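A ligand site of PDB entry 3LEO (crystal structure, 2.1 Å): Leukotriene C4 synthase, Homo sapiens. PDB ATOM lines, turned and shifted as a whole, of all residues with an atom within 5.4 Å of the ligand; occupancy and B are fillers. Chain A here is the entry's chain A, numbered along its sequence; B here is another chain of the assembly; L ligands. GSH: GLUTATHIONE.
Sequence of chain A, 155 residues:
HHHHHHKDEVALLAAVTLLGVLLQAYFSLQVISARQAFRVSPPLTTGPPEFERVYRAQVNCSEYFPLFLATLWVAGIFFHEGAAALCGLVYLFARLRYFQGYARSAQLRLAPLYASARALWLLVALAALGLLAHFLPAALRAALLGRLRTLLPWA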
ATOM      1  N   ARG A  56      -9.778 -10.290 -16.024  1.00  0.00           N
ATOM      2  CA  ARG A  56     -10.437  -9.024 -15.715  1.00  0.00           C
ATOM      3  C   ARG A  56     -10.733  -8.905 -14.228  1.00  0.00           C
ATOM      4  O   ARG A  56     -10.668  -7.790 -13.680  1.00  0.00           O
ATOM      5  CB  ARG A  56     -11.756  -8.860 -16.490  1.00  0.00           C
ATOM      6  CG  ARG A  56     -11.600  -8.537 -18.035  1.00  0.00           C
ATOM      7  CD  ARG A  56     -10.765  -7.276 -18.347  1.00  0.00           C
ATOM      8  NE  ARG A  56     -11.159  -6.179 -17.471  1.00  0.00           N
ATOM      9  CZ  ARG A  56     -10.395  -5.137 -17.131  1.00  0.00           C
ATOM     10  NH1 ARG A  56      -9.180  -4.972 -17.645  1.00  0.00           N
ATOM     11  NH2 ARG A  56     -10.863  -4.241 -16.258  1.00  0.00           N
ATOM     12  N   ALA A  57     -11.095 -10.025 -13.573  1.00  0.00           N
ATOM     13  CA  ALA A  57     -11.404  -9.952 -12.149  1.00  0.00           C
ATOM     14  C   ALA A  57     -10.170  -9.492 -11.351  1.00  0.00           C
ATOM     15  O   ALA A  57     -10.298  -8.713 -10.414  1.00  0.00           O
ATOM     16  CB  ALA A  57     -11.912 -11.283 -11.631  1.00  0.00           C
ATOM     17  N   ASN A  60      -9.408  -5.745 -12.215  1.00  0.00           N
ATOM     18  CA  ASN A  60     -10.322  -4.871 -11.482  1.00  0.00           C
ATOM     19  C   ASN A  60      -9.920  -4.715  -9.994  1.00  0.00           C
ATOM     20  O   ASN A  60      -9.891  -3.596  -9.487  1.00  0.00           O
ATOM     21  CB  ASN A  60     -11.780  -5.375 -11.613  1.00  0.00           C
ATOM     22  CG  ASN A  60     -12.824  -4.342 -11.169  1.00  0.00           C
ATOM     23  OD1 ASN A  60     -13.423  -3.629 -12.003  1.00  0.00           O
ATOM     24  ND2 ASN A  60     -13.039  -4.274  -9.870  1.00  0.00           N
ATOM     25  N   GLU A  63      -6.886  -2.469  -9.776  1.00  0.00           N
ATOM     26  CA  GLU A  63      -7.171  -1.017  -9.965  1.00  0.00           C
ATOM     27  C   GLU A  63      -7.667  -0.363  -8.722  1.00  0.00           C
ATOM     28  O   GLU A  63      -7.369   0.801  -8.465  1.00  0.00           O
ATOM     29  CB  GLU A  63      -8.344  -0.825 -10.934  1.00  0.00           C
ATOM     30  CG  GLU A  63      -7.939  -0.982 -12.266  1.00  0.00           C
ATOM     31  CD  GLU A  63      -9.053  -0.830 -13.257  1.00  0.00           C
ATOM     32  OE1 GLU A  63     -10.282  -0.824 -12.990  1.00  0.00           O
ATOM     33  OE2 GLU A  63      -8.628  -0.737 -14.362  1.00  0.00           O
ATOM     34  N   TYR A  64      -8.531  -1.076  -8.002  1.00  0.00           N
ATOM     35  CA  TYR A  64      -9.089  -0.528  -6.769  1.00  0.00           C
ATOM     36  C   TYR A  64      -8.218  -0.683  -5.538  1.00  0.00           C
ATOM     37  O   TYR A  64      -8.447   0.001  -4.527  1.00  0.00           O
ATOM     38  CB  TYR A  64     -10.431  -1.155  -6.472  1.00  0.00           C
ATOM     39  CG  TYR A  64     -11.549  -0.658  -7.354  1.00  0.00           C
ATOM     40  CD1 TYR A  64     -12.434   0.356  -6.922  1.00  0.00           C
ATOM     41  CD2 TYR A  64     -11.763  -1.216  -8.634  1.00  0.00           C
ATOM     42  CE1 TYR A  64     -13.506   0.805  -7.756  1.00  0.00           C
ATOM     43  CE2 TYR A  64     -12.799  -0.764  -9.448  1.00  0.00           C
ATOM     44  CZ  TYR A  64     -13.676   0.242  -8.989  1.00  0.00           C
ATOM     45  OH  TYR A  64     -14.724   0.652  -9.796  1.00  0.00           O
ATOM     46  N   TYR A  98     -16.001 -11.334  -5.117  1.00  0.00           N
ATOM     47  CA  TYR A  98     -16.091 -10.725  -6.453  1.00  0.00           C
ATOM     48  C   TYR A  98     -15.238 -11.516  -7.442  1.00  0.00           C
ATOM     49  O   TYR A  98     -15.688 -11.883  -8.552  1.00  0.00           O
ATOM     50  CB  TYR A  98     -15.631  -9.266  -6.379  1.00  0.00           C
ATOM     51  CG  TYR A  98     -15.443  -8.584  -7.722  1.00  0.00           C
ATOM     52  CD1 TYR A  98     -16.504  -7.939  -8.357  1.00  0.00           C
ATOM     53  CD2 TYR A  98     -14.191  -8.587  -8.358  1.00  0.00           C
ATOM     54  CE1 TYR A  98     -16.333  -7.304  -9.592  1.00  0.00           C
ATOM     55  CE2 TYR A  98     -14.015  -7.954  -9.627  1.00  0.00           C
ATOM     56  CZ  TYR A  98     -15.091  -7.321 -10.213  1.00  0.00           C
ATOM     57  OH  TYR A  98     -14.963  -6.665 -11.398  1.00  0.00           O
ATOM     58  N   TYR A 102     -17.100 -13.525 -10.437  1.00  0.00           N
ATOM     59  CA  TYR A 102     -16.754 -13.062 -11.779  1.00  0.00           C
ATOM     60  C   TYR A 102     -16.077 -14.210 -12.584  1.00  0.00           C
ATOM     61  O   TYR A 102     -16.422 -14.439 -13.733  1.00  0.00           O
ATOM     62  CB  TYR A 102     -15.836 -11.835 -11.673  1.00  0.00           C
ATOM     63  CG  TYR A 102     -15.637 -10.963 -12.911  1.00  0.00           C
ATOM     64  CD1 TYR A 102     -14.902  -9.770 -12.818  1.00  0.00           C
ATOM     65  CD2 TYR A 102     -16.188 -11.299 -14.148  1.00  0.00           C
ATOM     66  CE1 TYR A 102     -14.675  -8.950 -13.948  1.00  0.00           C
ATOM     67  CE2 TYR A 102     -15.979 -10.465 -15.284  1.00  0.00           C
ATOM     68  CZ  TYR A 102     -15.224  -9.318 -15.180  1.00  0.00           C
ATOM     69  OH  TYR A 102     -15.042  -8.490 -16.286  1.00  0.00           O
ATOM     70  N   ARG A 109     -20.376 -11.433 -10.469  1.00  0.00           N
ATOM     71  CA  ARG A 109     -19.521 -10.371  -9.914  1.00  0.00           C
ATOM     72  C   ARG A 109     -20.328  -9.275  -9.190  1.00  0.00           C
ATOM     73  O   ARG A 109     -19.765  -8.566  -8.349  1.00  0.00           O
ATOM     74  CB  ARG A 109     -18.666  -9.713 -11.009  1.00  0.00           C
ATOM     75  CG  ARG A 109     -19.356  -8.511 -11.702  1.00  0.00           C
ATOM     76  CD  ARG A 109     -18.613  -8.071 -12.963  1.00  0.00           C
ATOM     77  NE  ARG A 109     -19.151  -6.826 -13.508  1.00  0.00           N
ATOM     78  CZ  ARG A 109     -20.252  -6.786 -14.274  1.00  0.00           C
ATOM     79  NH1 ARG A 109     -20.721  -5.626 -14.719  1.00  0.00           N
ATOM     80  NH2 ARG A 109     -20.928  -7.919 -14.576  1.00  0.00           N
ATOM     81  N   LEU A 110     -21.622  -9.138  -9.519  1.00  0.00           N
ATOM     82  CA  LEU A 110     -22.378  -7.911  -9.189  1.00  0.00           C
ATOM     83  C   LEU A 110     -22.718  -7.769  -7.698  1.00  0.00           C
ATOM     84  O   LEU A 110     -22.427  -6.748  -7.095  1.00  0.00           O
ATOM     85  CB  LEU A 110     -23.633  -7.778 -10.064  1.00  0.00           C
ATOM     86  CG  LEU A 110     -23.364  -7.508 -11.560  1.00  0.00           C
ATOM     87  CD1 LEU A 110     -24.668  -7.724 -12.435  1.00  0.00           C
ATOM     88  CD2 LEU A 110     -22.721  -6.124 -11.729  1.00  0.00           C
ATOM     89  N   LEU A 113     -19.470  -7.134  -5.849  1.00  0.00           N
ATOM     90  CA  LEU A 113     -19.017  -5.779  -6.242  1.00  0.00           C
ATOM     91  C   LEU A 113     -19.750  -4.713  -5.427  1.00  0.00           C
ATOM     92  O   LEU A 113     -19.113  -3.795  -4.928  1.00  0.00           O
ATOM     93  CB  LEU A 113     -19.219  -5.491  -7.743  1.00  0.00           C
ATOM     94  CG  LEU A 113     -18.875  -4.037  -8.127  1.00  0.00           C
ATOM     95  CD1 LEU A 113     -17.343  -3.713  -7.926  1.00  0.00           C
ATOM     96  CD2 LEU A 113     -19.347  -3.770  -9.546  1.00  0.00           C
ATOM     97  N   SER B  28     -14.184   5.798 -12.319  1.00  0.00           N
ATOM     98  CA  SER B  28     -14.796   4.460 -12.331  1.00  0.00           C
ATOM     99  C   SER B  28     -16.304   4.507 -12.610  1.00  0.00           C
ATOM    100  O   SER B  28     -16.810   3.716 -13.392  1.00  0.00           O
ATOM    101  CB  SER B  28     -14.550   3.711 -11.024  1.00  0.00           C
ATOM    102  OG  SER B  28     -13.163   3.505 -10.892  1.00  0.00           O
ATOM    103  N   VAL B  31     -16.830   5.165 -16.319  1.00  0.00           N
ATOM    104  CA  VAL B  31     -16.694   3.924 -17.122  1.00  0.00           C
ATOM    105  C   VAL B  31     -17.974   3.047 -17.033  1.00  0.00           C
ATOM    106  O   VAL B  31     -18.455   2.525 -18.054  1.00  0.00           O
ATOM    107  CB  VAL B  31     -15.454   3.099 -16.721  1.00  0.00           C
ATOM    108  CG1 VAL B  31     -15.404   1.794 -17.493  1.00  0.00           C
ATOM    109  CG2 VAL B  31     -14.182   3.917 -16.979  1.00  0.00           C
ATOM    110  N   ILE B  32     -18.499   2.822 -15.827  1.00  0.00           N
ATOM    111  CA  ILE B  32     -19.748   2.004 -15.660  1.00  0.00           C
ATOM    112  C   ILE B  32     -20.851   2.639 -16.516  1.00  0.00           C
ATOM    113  O   ILE B  32     -21.610   1.942 -17.228  1.00  0.00           O
ATOM    114  CB  ILE B  32     -20.161   1.954 -14.170  1.00  0.00           C
ATOM    115  CG1 ILE B  32     -19.099   1.198 -13.352  1.00  0.00           C
ATOM    116  CG2 ILE B  32     -21.559   1.290 -14.027  1.00  0.00           C
ATOM    117  CD1 ILE B  32     -19.243   1.316 -11.830  1.00  0.00           C
ATOM    118  N   ARG B  35     -20.185   1.909 -20.194  1.00  0.00           N
ATOM    119  CA  ARG B  35     -20.617   0.513 -20.436  1.00  0.00           C
ATOM    120  C   ARG B  35     -22.116   0.398 -20.733  1.00  0.00           C
ATOM    121  O   ARG B  35     -22.504  -0.323 -21.657  1.00  0.00           O
ATOM    122  CB  ARG B  35     -20.247  -0.420 -19.253  1.00  0.00           C
ATOM    123  CG  ARG B  35     -18.766  -0.759 -19.158  1.00  0.00           C
ATOM    124  CD  ARG B  35     -18.451  -1.819 -18.103  1.00  0.00           C
ATOM    125  NE  ARG B  35     -17.013  -2.128 -18.070  1.00  0.00           N
ATOM    126  CZ  ARG B  35     -16.394  -2.928 -18.956  1.00  0.00           C
ATOM    127  NH1 ARG B  35     -17.087  -3.482 -19.949  1.00  0.00           N
ATOM    128  NH2 ARG B  35     -15.088  -3.156 -18.873  1.00  0.00           N
ATOM    129  N   PRO B  42     -18.848  -6.468 -19.313  1.00  0.00           N
ATOM    130  CA  PRO B  42     -17.695  -7.264 -18.883  1.00  0.00           C
ATOM    131  C   PRO B  42     -17.850  -8.722 -19.324  1.00  0.00           C
ATOM    132  O   PRO B  42     -18.984  -9.222 -19.373  1.00  0.00           O
ATOM    133  CB  PRO B  42     -17.733  -7.114 -17.355  1.00  0.00           C
ATOM    134  CG  PRO B  42     -18.340  -5.702 -17.182  1.00  0.00           C
ATOM    135  CD  PRO B  42     -19.483  -5.754 -18.177  1.00  0.00           C
ATOM    136  N   PRO B  43     -16.751  -9.414 -19.663  1.00  0.00           N
ATOM    137  CA  PRO B  43     -15.339  -9.019 -19.534  1.00  0.00           C
ATOM    138  C   PRO B  43     -14.754  -8.150 -20.681  1.00  0.00           C
ATOM    139  O   PRO B  43     -13.531  -7.945 -20.685  1.00  0.00           O
ATOM    140  CB  PRO B  43     -14.633 -10.369 -19.467  1.00  0.00           C
ATOM    141  CG  PRO B  43     -15.444 -11.278 -20.416  1.00  0.00           C
ATOM    142  CD  PRO B  43     -16.903 -10.776 -20.232  1.00  0.00           C
ATOM    143  N   THR B  45     -13.365  -5.101 -22.821  1.00  0.00           N
ATOM    144  CA  THR B  45     -12.836  -3.732 -22.626  1.00  0.00           C
ATOM    145  C   THR B  45     -12.600  -3.018 -23.983  1.00  0.00           C
ATOM    146  O   THR B  45     -11.929  -1.969 -24.073  1.00  0.00           O
ATOM    147  CB  THR B  45     -11.570  -3.722 -21.783  1.00  0.00           C
ATOM    148  OG1 THR B  45     -10.567  -4.545 -22.422  1.00  0.00           O
ATOM    149  CG2 THR B  45     -11.864  -4.253 -20.393  1.00  0.00           C
ATOM    150  N   TYR B  55     -12.741   4.200 -21.069  1.00  0.00           N
ATOM    151  CA  TYR B  55     -12.067   3.078 -20.402  1.00  0.00           C
ATOM    152  C   TYR B  55     -10.584   3.400 -20.217  1.00  0.00           C
ATOM    153  O   TYR B  55     -10.048   3.323 -19.102  1.00  0.00           O
ATOM    154  CB  TYR B  55     -12.246   1.772 -21.215  1.00  0.00           C
ATOM    155  CG  TYR B  55     -11.373   0.669 -20.714  1.00  0.00           C
ATOM    156  CD1 TYR B  55     -11.697  -0.021 -19.538  1.00  0.00           C
ATOM    157  CD2 TYR B  55     -10.202   0.332 -21.398  1.00  0.00           C
ATOM    158  CE1 TYR B  55     -10.865  -1.015 -19.046  1.00  0.00           C
ATOM    159  CE2 TYR B  55      -9.358  -0.691 -20.918  1.00  0.00           C
ATOM    160  CZ  TYR B  55      -9.701  -1.335 -19.753  1.00  0.00           C
ATOM    161  OH  TYR B  55      -8.888  -2.298 -19.254  1.00  0.00           O
ATOM    162  N   GLN B  58      -9.585   6.245 -17.696  1.00  0.00           N
ATOM    163  CA  GLN B  58      -9.685   5.777 -16.327  1.00  0.00           C
ATOM    164  C   GLN B  58      -8.501   4.868 -15.986  1.00  0.00           C
ATOM    165  O   GLN B  58      -7.882   5.039 -14.934  1.00  0.00           O
ATOM    166  CB  GLN B  58     -11.007   4.999 -16.088  1.00  0.00           C
ATOM    167  CG  GLN B  58     -11.072   4.346 -14.660  1.00  0.00           C
ATOM    168  CD  GLN B  58     -10.753   2.876 -14.688  1.00  0.00           C
ATOM    169  OE1 GLN B  58      -9.811   2.411 -14.032  1.00  0.00           O
ATOM    170  NE2 GLN B  58     -11.514   2.143 -15.456  1.00  0.00           N
ATOM    171  N   VAL B  59      -8.180   3.917 -16.881  1.00  0.00           N
ATOM    172  CA  VAL B  59      -7.083   2.982 -16.650  1.00  0.00           C
ATOM    173  C   VAL B  59      -5.739   3.757 -16.567  1.00  0.00           C
ATOM    174  O   VAL B  59      -4.917   3.438 -15.722  1.00  0.00           O
ATOM    175  CB  VAL B  59      -7.017   1.942 -17.759  1.00  0.00           C
ATOM    176  CG1 VAL B  59      -5.696   1.106 -17.618  1.00  0.00           C
ATOM    177  CG2 VAL B  59      -8.253   0.994 -17.650  1.00  0.00           C
HETATM  178  N1  GSH L   1     -12.059  -0.838 -15.080  1.00  0.00           N
HETATM  179  CA1 GSH L   1     -13.396  -0.333 -15.142  1.00  0.00           C
HETATM  180  C1  GSH L   1     -14.179  -1.282 -16.027  1.00  0.00           C
HETATM  181  O11 GSH L   1     -15.363  -1.674 -15.882  1.00  0.00           O
HETATM  182  O12 GSH L   1     -13.579  -1.639 -17.056  1.00  0.00           O
HETATM  183  CB1 GSH L   1     -13.963   0.329 -13.865  1.00  0.00           C
HETATM  184  CG1 GSH L   1     -15.485   0.433 -13.768  1.00  0.00           C
HETATM  185  CD1 GSH L   1     -15.858  -0.774 -12.895  1.00  0.00           C
HETATM  186  OE1 GSH L   1     -15.100  -1.106 -11.787  1.00  0.00           O
HETATM  187  N2  GSH L   1     -16.878  -1.540 -13.266  1.00  0.00           N
HETATM  188  CA2 GSH L   1     -17.402  -2.723 -12.560  1.00  0.00           C
HETATM  189  C2  GSH L   1     -16.768  -4.010 -13.061  1.00  0.00           C
HETATM  190  O2  GSH L   1     -17.013  -5.192 -12.437  1.00  0.00           O
HETATM  191  CB2 GSH L   1     -18.904  -2.764 -12.820  1.00  0.00           C
HETATM  192  SG2 GSH L   1     -19.261  -2.866 -14.607  1.00  0.00           S
HETATM  193  N3  GSH L   1     -15.928  -4.008 -14.102  1.00  0.00           N
HETATM  194  CA3 GSH L   1     -15.510  -5.245 -14.765  1.00  0.00           C
HETATM  195  C3  GSH L   1     -14.055  -5.234 -15.161  1.00  0.00           C
HETATM  196  O31 GSH L   1     -13.261  -4.314 -14.797  1.00  0.00           O
HETATM  197  O32 GSH L   1     -13.632  -6.183 -15.896  1.00  0.00           O
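The side-chain carboxylate (OE2) of Glu 63 sits close to the side-chain amide oxygen (OE1) of Gln 58 of chain B, at 3.4 Å. OH of Tyr 98 sits close to ND2 of Asn 60 (3.4 Å). OG of Ser 28 of chain B sits close to OH of Tyr 64, at 3.4 Å. OH of Tyr 55 of chain B lies within hydrogen-bond range of NH1 of Arg 56 (3.1 Å).
An oxygen (O32) of the ligand lies within hydrogen-bond range of the side-chain hydroxyl (OH) of Tyr 102 (2.7 Å). The side-chain hydroxyl of Tyr 64 sits at hydrogen-bond distance from an oxygen (OE1) of the ligand. An oxygen (O2) of the ligand sits at hydrogen-bond distance from the side-chain hydroxyl (OH) of Tyr 98. A nitrogen (N1) of the ligand sits close to the side-chain amide nitrogen of Gln 58 of chain B, at 3.1 Å. An oxygen (O31) of the ligand lies close to the side-chain amide oxygen (OD1) of Asn 60, at 2.9 Å. NE of Arg 35 of chain B lies within salt-bridge range of O11 of the ligand (2.8 Å). The guanidinium group (NE) of Arg 109 lies within hydrogen-bond range of an oxygen (O2) of the ligand. The guanidinium group (NH2) of Arg 56 lies within salt-bridge range of an oxygen (O31) of the ligand, 2.8 Å away. The side-chain carboxylate (OE1) of Glu 63 is in salt-bridge range of a nitrogen (N1) of the ligand, 2.7 Å away.
Leu 113 touches the ligand (CD2 to CB2, 3.5 Å). Ser 28 of chain B touches the ligand (O to CG1, 3.6 Å). Val 31 of chain B touches the ligand. Ile 32 of chain B touches the ligand (CG1 to N2, 3.5 Å). Pro 42 of chain B touches the ligand (CG to CA3, 3.7 Å). Tyr 55 of chain B touches the ligand. Hydrophobic or aromatic side chains that line the ligand: Tyr 64, Tyr 98, Tyr 102, Leu 113, Val 31 of chain B, Ile 32 of chain B, Pro 42 of chain B and Tyr 55 of chain B. 15 residues have an atom within 4 Å of the ligand: Arg 56, Asn 60, Glu 63, Tyr 64, Tyr 98, Tyr 102, Arg 109, Leu 113, Ser 28 of chain B, Val 31 of chain B, Ile 32 of chain B, Arg 35 of chain B, Pro 42 of chain B, Tyr 55 of chain B and Gln 58 of chain B. The nearest printed residue that does not touch the ligand is Thr 45 of chain B (4.6 Å).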
